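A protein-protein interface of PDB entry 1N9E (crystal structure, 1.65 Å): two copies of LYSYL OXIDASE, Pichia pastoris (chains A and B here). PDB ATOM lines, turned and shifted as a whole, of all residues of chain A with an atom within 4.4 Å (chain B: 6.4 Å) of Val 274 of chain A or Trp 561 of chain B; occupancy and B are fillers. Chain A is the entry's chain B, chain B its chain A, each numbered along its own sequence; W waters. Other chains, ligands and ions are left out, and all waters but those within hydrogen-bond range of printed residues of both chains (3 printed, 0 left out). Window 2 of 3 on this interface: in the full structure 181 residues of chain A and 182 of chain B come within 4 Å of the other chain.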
ATOM      1  N   TYR A 230      -3.755   1.278  -9.385  1.00  0.00           N
ATOM      2  CA  TYR A 230      -3.760   2.602  -9.972  1.00  0.00           C
ATOM      3  C   TYR A 230      -3.610   3.612  -8.848  1.00  0.00           C
ATOM      4  O   TYR A 230      -3.732   3.262  -7.665  1.00  0.00           O
ATOM      5  CB  TYR A 230      -5.072   2.851 -10.755  1.00  0.00           C
ATOM      6  CG  TYR A 230      -5.119   2.073 -12.058  1.00  0.00           C
ATOM      7  CD1 TYR A 230      -5.538   0.741 -12.084  1.00  0.00           C
ATOM      8  CD2 TYR A 230      -4.742   2.670 -13.252  1.00  0.00           C
ATOM      9  CE1 TYR A 230      -5.581   0.034 -13.270  1.00  0.00           C
ATOM     10  CE2 TYR A 230      -4.779   1.974 -14.448  1.00  0.00           C
ATOM     11  CZ  TYR A 230      -5.201   0.652 -14.445  1.00  0.00           C
ATOM     12  OH  TYR A 230      -5.237  -0.036 -15.640  1.00  0.00           O
ATOM     13  N   GLU A 267       2.565   2.696 -15.975  1.00  0.00           N
ATOM     14  CA  GLU A 267       2.006   3.763 -16.792  1.00  0.00           C
ATOM     15  C   GLU A 267       1.830   5.053 -16.037  1.00  0.00           C
ATOM     16  O   GLU A 267       1.578   5.046 -14.825  1.00  0.00           O
ATOM     17  CB  GLU A 267       0.604   3.365 -17.309  1.00  0.00           C
ATOM     18  CG  GLU A 267       0.549   2.053 -18.073  1.00  0.00           C
ATOM     19  CD  GLU A 267      -0.873   1.633 -18.448  1.00  0.00           C
ATOM     20  OE1 GLU A 267      -1.014   0.791 -19.363  1.00  0.00           O
ATOM     21  OE2 GLU A 267      -1.848   2.133 -17.842  1.00  0.00           O
ATOM     22  N   TYR A 268       1.969   6.152 -16.776  1.00  0.00           N
ATOM     23  CA  TYR A 268       1.466   7.440 -16.338  1.00  0.00           C
ATOM     24  C   TYR A 268       0.293   7.771 -17.266  1.00  0.00           C
ATOM     25  O   TYR A 268       0.372   7.585 -18.492  1.00  0.00           O
ATOM     26  CB  TYR A 268       2.567   8.528 -16.393  1.00  0.00           C
ATOM     27  CG  TYR A 268       3.598   8.250 -15.330  1.00  0.00           C
ATOM     28  CD1 TYR A 268       4.851   7.772 -15.657  1.00  0.00           C
ATOM     29  CD2 TYR A 268       3.305   8.465 -13.980  1.00  0.00           C
ATOM     30  CE1 TYR A 268       5.802   7.510 -14.668  1.00  0.00           C
ATOM     31  CE2 TYR A 268       4.247   8.209 -12.991  1.00  0.00           C
ATOM     32  CZ  TYR A 268       5.483   7.733 -13.338  1.00  0.00           C
ATOM     33  OH  TYR A 268       6.419   7.480 -12.335  1.00  0.00           O
ATOM     34  N   ILE A 269      -0.792   8.260 -16.685  1.00  0.00           N
ATOM     35  CA  ILE A 269      -1.992   8.556 -17.461  1.00  0.00           C
ATOM     36  C   ILE A 269      -2.413   9.990 -17.215  1.00  0.00           C
ATOM     37  O   ILE A 269      -2.609  10.404 -16.067  1.00  0.00           O
ATOM     38  CB  ILE A 269      -3.124   7.577 -17.092  1.00  0.00           C
ATOM     39  CG1 ILE A 269      -2.707   6.142 -17.440  1.00  0.00           C
ATOM     40  CG2 ILE A 269      -4.392   7.934 -17.869  1.00  0.00           C
ATOM     41  CD1 ILE A 269      -3.509   5.063 -16.691  1.00  0.00           C
ATOM     42  N   ASN A 272      -6.230  11.404 -20.613  1.00  0.00           N
ATOM     43  CA  ASN A 272      -6.655  10.188 -21.314  1.00  0.00           C
ATOM     44  C   ASN A 272      -5.618   9.563 -22.238  1.00  0.00           C
ATOM     45  O   ASN A 272      -5.955   8.732 -23.078  1.00  0.00           O
ATOM     46  CB  ASN A 272      -7.997  10.404 -22.032  1.00  0.00           C
ATOM     47  CG  ASN A 272      -9.145  10.483 -21.056  1.00  0.00           C
ATOM     48  OD1 ASN A 272      -9.380   9.534 -20.290  1.00  0.00           O
ATOM     49  ND2 ASN A 272      -9.866  11.603 -21.064  1.00  0.00           N
ATOM     50  N   LYS A 273      -4.361   9.972 -22.079  1.00  0.00           N
ATOM     51  CA  LYS A 273      -3.274   9.395 -22.847  1.00  0.00           C
ATOM     52  C   LYS A 273      -2.385   8.597 -21.905  1.00  0.00           C
ATOM     53  O   LYS A 273      -2.209   8.981 -20.755  1.00  0.00           O
ATOM     54  CB  LYS A 273      -2.444  10.498 -23.509  1.00  0.00           C
ATOM     55  CG  LYS A 273      -3.273  11.401 -24.432  1.00  0.00           C
ATOM     56  CD  LYS A 273      -2.358  12.288 -25.269  1.00  0.00           C
ATOM     57  CE  LYS A 273      -3.159  13.272 -26.112  1.00  0.00           C
ATOM     58  NZ  LYS A 273      -4.159  12.601 -26.977  1.00  0.00           N
ATOM     59  N   VAL A 274      -1.836   7.498 -22.417  1.00  0.00           N
ATOM     60  CA  VAL A 274      -1.004   6.571 -21.650  1.00  0.00           C
ATOM     61  C   VAL A 274       0.470   6.690 -22.041  1.00  0.00           C
ATOM     62  O   VAL A 274       0.811   6.665 -23.229  1.00  0.00           O
ATOM     63  CB  VAL A 274      -1.445   5.111 -21.893  1.00  0.00           C
ATOM     64  CG1 VAL A 274      -0.631   4.133 -21.042  1.00  0.00           C
ATOM     65  CG2 VAL A 274      -2.926   4.952 -21.613  1.00  0.00           C
ATOM     66  N   TYR A 275       1.332   6.820 -21.035  1.00  0.00           N
ATOM     67  CA  TYR A 275       2.785   6.877 -21.235  1.00  0.00           C
ATOM     68  C   TYR A 275       3.395   5.710 -20.467  1.00  0.00           C
ATOM     69  O   TYR A 275       3.007   5.456 -19.326  1.00  0.00           O
ATOM     70  CB  TYR A 275       3.356   8.241 -20.734  1.00  0.00           C
ATOM     71  CG  TYR A 275       2.630   9.374 -21.424  1.00  0.00           C
ATOM     72  CD1 TYR A 275       1.438   9.880 -20.905  1.00  0.00           C
ATOM     73  CD2 TYR A 275       3.127   9.936 -22.601  1.00  0.00           C
ATOM     74  CE1 TYR A 275       0.765  10.909 -21.533  1.00  0.00           C
ATOM     75  CE2 TYR A 275       2.465  10.962 -23.235  1.00  0.00           C
ATOM     76  CZ  TYR A 275       1.288  11.448 -22.706  1.00  0.00           C
ATOM     77  OH  TYR A 275       0.631  12.471 -23.342  1.00  0.00           O
ATOM     78  N   THR A 276       4.341   4.998 -21.071  1.00  0.00           N
ATOM     79  CA  THR A 276       4.910   3.822 -20.419  1.00  0.00           C
ATOM     80  C   THR A 276       6.144   4.108 -19.590  1.00  0.00           C
ATOM     81  O   THR A 276       6.711   3.193 -18.987  1.00  0.00           O
ATOM     82  CB  THR A 276       5.220   2.711 -21.416  1.00  0.00           C
ATOM     83  OG1 THR A 276       5.960   3.252 -22.521  1.00  0.00           O
ATOM     84  CG2 THR A 276       3.910   2.189 -22.037  1.00  0.00           C
ATOM     85  N   ASP A 387     -14.799   8.275 -15.661  1.00  0.00           N
ATOM     86  CA  ASP A 387     -13.992   8.207 -16.879  1.00  0.00           C
ATOM     87  C   ASP A 387     -12.524   7.982 -16.580  1.00  0.00           C
ATOM     88  O   ASP A 387     -11.750   7.672 -17.497  1.00  0.00           O
ATOM     89  CB  ASP A 387     -14.096   9.504 -17.698  1.00  0.00           C
ATOM     90  CG  ASP A 387     -13.749  10.769 -16.904  1.00  0.00           C
ATOM     91  OD1 ASP A 387     -13.999  10.823 -15.678  1.00  0.00           O
ATOM     92  OD2 ASP A 387     -13.222  11.782 -17.445  1.00  0.00           O
ATOM     93  N   ASP A 388     -12.141   8.136 -15.311  1.00  0.00           N
ATOM     94  CA  ASP A 388     -10.717   8.150 -14.959  1.00  0.00           C
ATOM     95  C   ASP A 388     -10.308   6.873 -14.237  1.00  0.00           C
ATOM     96  O   ASP A 388     -11.162   6.214 -13.629  1.00  0.00           O
ATOM     97  CB  ASP A 388     -10.315   9.494 -14.269  1.00  0.00           C
ATOM     98  CG  ASP A 388     -10.548   9.524 -12.748  1.00  0.00           C
ATOM     99  OD1 ASP A 388     -11.033  10.595 -12.249  1.00  0.00           O
ATOM    100  OD2 ASP A 388     -10.276   8.554 -11.989  1.00  0.00           O
ATOM    101  N   PRO A 389      -9.023   6.503 -14.307  1.00  0.00           N
ATOM    102  CA  PRO A 389      -8.557   5.248 -13.693  1.00  0.00           C
ATOM    103  C   PRO A 389      -8.364   5.233 -12.200  1.00  0.00           C
ATOM    104  O   PRO A 389      -7.949   4.192 -11.680  1.00  0.00           O
ATOM    105  CB  PRO A 389      -7.209   4.993 -14.394  1.00  0.00           C
ATOM    106  CG  PRO A 389      -6.700   6.364 -14.755  1.00  0.00           C
ATOM    107  CD  PRO A 389      -7.932   7.230 -14.988  1.00  0.00           C
ATOM    108  N   HIS A 393     -11.596   2.710 -10.517  1.00  0.00           N
ATOM    109  CA  HIS A 393     -11.042   1.573  -9.772  1.00  0.00           C
ATOM    110  C   HIS A 393     -11.262   1.653  -8.267  1.00  0.00           C
ATOM    111  O   HIS A 393     -10.600   0.968  -7.511  1.00  0.00           O
ATOM    112  CB  HIS A 393      -9.561   1.331 -10.104  1.00  0.00           C
ATOM    113  CG  HIS A 393      -9.350   0.930 -11.526  1.00  0.00           C
ATOM    114  ND1 HIS A 393      -8.736   1.751 -12.447  1.00  0.00           N
ATOM    115  CD2 HIS A 393      -9.678  -0.205 -12.189  1.00  0.00           C
ATOM    116  CE1 HIS A 393      -8.694   1.141 -13.617  1.00  0.00           C
ATOM    117  NE2 HIS A 393      -9.257  -0.046 -13.490  1.00  0.00           N
ATOM    118  N   TYR B 559     -12.287   2.281 -22.089  1.00  0.00           N
ATOM    119  CA  TYR B 559     -11.652   3.566 -21.847  1.00  0.00           C
ATOM    120  C   TYR B 559     -10.377   3.743 -22.673  1.00  0.00           C
ATOM    121  O   TYR B 559      -9.685   2.772 -22.943  1.00  0.00           O
ATOM    122  CB  TYR B 559     -11.255   3.641 -20.391  1.00  0.00           C
ATOM    123  CG  TYR B 559     -12.410   3.606 -19.425  1.00  0.00           C
ATOM    124  CD1 TYR B 559     -12.693   2.455 -18.684  1.00  0.00           C
ATOM    125  CD2 TYR B 559     -13.212   4.726 -19.251  1.00  0.00           C
ATOM    126  CE1 TYR B 559     -13.753   2.416 -17.793  1.00  0.00           C
ATOM    127  CE2 TYR B 559     -14.280   4.704 -18.357  1.00  0.00           C
ATOM    128  CZ  TYR B 559     -14.540   3.546 -17.635  1.00  0.00           C
ATOM    129  OH  TYR B 559     -15.597   3.538 -16.754  1.00  0.00           O
ATOM    130  N   PRO B 560     -10.058   4.970 -23.077  1.00  0.00           N
ATOM    131  CA  PRO B 560      -8.820   5.211 -23.840  1.00  0.00           C
ATOM    132  C   PRO B 560      -7.548   4.775 -23.134  1.00  0.00           C
ATOM    133  O   PRO B 560      -6.555   4.449 -23.801  1.00  0.00           O
ATOM    134  CB  PRO B 560      -8.850   6.725 -24.107  1.00  0.00           C
ATOM    135  CG  PRO B 560      -9.748   7.276 -23.024  1.00  0.00           C
ATOM    136  CD  PRO B 560     -10.824   6.217 -22.869  1.00  0.00           C
ATOM    137  N   TRP B 561      -7.571   4.767 -21.807  1.00  0.00           N
ATOM    138  CA  TRP B 561      -6.377   4.381 -21.063  1.00  0.00           C
ATOM    139  C   TRP B 561      -6.262   2.869 -20.836  1.00  0.00           C
ATOM    140  O   TRP B 561      -5.319   2.417 -20.206  1.00  0.00           O
ATOM    141  CB  TRP B 561      -6.299   5.163 -19.732  1.00  0.00           C
ATOM    142  CG  TRP B 561      -7.605   5.259 -18.965  1.00  0.00           C
ATOM    143  CD1 TRP B 561      -8.450   6.341 -18.896  1.00  0.00           C
ATOM    144  CD2 TRP B 561      -8.214   4.230 -18.159  1.00  0.00           C
ATOM    145  NE1 TRP B 561      -9.535   6.043 -18.102  1.00  0.00           N
ATOM    146  CE2 TRP B 561      -9.416   4.758 -17.638  1.00  0.00           C
ATOM    147  CE3 TRP B 561      -7.859   2.918 -17.829  1.00  0.00           C
ATOM    148  CZ2 TRP B 561     -10.266   4.014 -16.801  1.00  0.00           C
ATOM    149  CZ3 TRP B 561      -8.697   2.180 -17.005  1.00  0.00           C
ATOM    150  CH2 TRP B 561      -9.891   2.736 -16.501  1.00  0.00           C
ATOM    151  N   ALA B 562      -7.212   2.074 -21.339  1.00  0.00           N
ATOM    152  CA  ALA B 562      -7.050   0.602 -21.277  1.00  0.00           C
ATOM    153  C   ALA B 562      -7.699   0.014 -22.515  1.00  0.00           C
ATOM    154  O   ALA B 562      -8.752  -0.610 -22.464  1.00  0.00           O
ATOM    155  CB  ALA B 562      -7.656   0.010 -19.995  1.00  0.00           C
ATOM    156  N   PRO B 563      -7.068   0.214 -23.658  1.00  0.00           N
ATOM    157  CA  PRO B 563      -7.710  -0.177 -24.913  1.00  0.00           C
ATOM    158  C   PRO B 563      -8.047  -1.661 -24.923  1.00  0.00           C
ATOM    159  O   PRO B 563      -7.248  -2.480 -24.491  1.00  0.00           O
ATOM    160  CB  PRO B 563      -6.630   0.110 -25.966  1.00  0.00           C
ATOM    161  CG  PRO B 563      -5.706   1.101 -25.313  1.00  0.00           C
ATOM    162  CD  PRO B 563      -5.732   0.810 -23.846  1.00  0.00           C
ATOM    163  N   TYR B 567     -15.268  -2.632 -19.399  1.00  0.00           N
ATOM    164  CA  TYR B 567     -15.648  -2.492 -18.007  1.00  0.00           C
ATOM    165  C   TYR B 567     -17.156  -2.344 -17.922  1.00  0.00           C
ATOM    166  O   TYR B 567     -17.768  -1.635 -18.731  1.00  0.00           O
ATOM    167  CB  TYR B 567     -15.088  -1.201 -17.418  1.00  0.00           C
ATOM    168  CG  TYR B 567     -13.642  -1.214 -17.020  1.00  0.00           C
ATOM    169  CD1 TYR B 567     -12.640  -1.138 -17.981  1.00  0.00           C
ATOM    170  CD2 TYR B 567     -13.283  -1.297 -15.685  1.00  0.00           C
ATOM    171  CE1 TYR B 567     -11.303  -1.147 -17.608  1.00  0.00           C
ATOM    172  CE2 TYR B 567     -11.966  -1.308 -15.306  1.00  0.00           C
ATOM    173  CZ  TYR B 567     -10.982  -1.233 -16.265  1.00  0.00           C
ATOM    174  OH  TYR B 567      -9.666  -1.246 -15.833  1.00  0.00           O
HETATM  175  O   HOH W   1      -3.050   1.067 -21.119  1.00  0.00           O
HETATM  176  O   HOH W   2      -4.339   1.211 -17.902  1.00  0.00           O
HETATM  177  O   HOH W   3      -7.224  -1.867 -16.756  1.00  0.00           O
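Among the printed residues, merely in contact across the chains: His 393 of chain A with Trp 561 of chain B, Val 274 of chain A with Trp 561 of chain B, Asn 272 of chain A with Pro 560 of chain B, Asn 272 of chain A with Trp 561 of chain B, Pro 389 of chain A with Trp 561 of chain B, Asp 387 of chain A with Tyr 559 of chain B, Asp 388 of chain A with Trp 561 of chain B and Ile 269 of chain A with Trp 561 of chain B.
Water W2 lies within hydrogen-bond range of OE2 of Glu 267 of chain A (2.7 Å), OH of Tyr 230 of chain A (2.7 Å) and O of Trp 561 of chain B (2.8 Å).
Water W3 lies within hydrogen-bond range of OH of Tyr 567 of chain B (2.7 Å) and OH of Tyr 230 of chain A (2.9 Å).
Water W1 bridges OE1 of Glu 267 of chain A (2.7 Å) and O of Trp 561 of chain B (2.8 Å).
The indole nitrogen of Trp 561 of chain B sits at hydrogen-bond distance from the backbone carbonyl oxygen of Asp 387 of chain A (2.8 Å).
A ring nitrogen (NE2) of His 393 of chain A lies within hydrogen-bond range of the side-chain hydroxyl (OH) of Tyr 567 of chain B.
Hydrophobic or aromatic side chains of chain B within 4 Å of the printed part of chain A: Tyr 559, Pro 560, Trp 561 and Tyr 567.
Of the 13 printed residues of chain A, 7 touch a printed residue of chain B.
Hydrophobic or aromatic side chains of chain A that line the printed part of chain B: Ile 269, Val 274, Pro 389 and His 393.
Among the printed residues, no Asp or Glu carboxylate lies within 4 Å of a Lys or Arg side-chain nitrogen of the other chain.
Of chain B, only Trp 561 (3.5 Å) comes within 4 Å of Val 274 of chain A.
Of the printed residues of chain A, Tyr 567 of chain B touches His 393 (2.7 Å).
Printed residues of chain B within 4 Å of Pro 389 of chain A: Trp 561 (3.7 Å).
The nearest residue of chain B that does not touch Val 274 of chain A is Pro 560 of chain B (4.3 Å).
The nearest residue of chain A that does not touch Trp 561 of chain B is Glu 267 of chain A (4.2 Å).
The nearest printed residue of chain B that does not touch Pro 389 of chain A is Tyr 559 of chain B (6.7 Å).
A ring nitrogen (ND1) of His 393 of chain A is in hydrogen-bond range of the backbone carbonyl oxygen (O) of Pro 389 of chain A, 2.7 Å away.
No position is printed for both chains.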
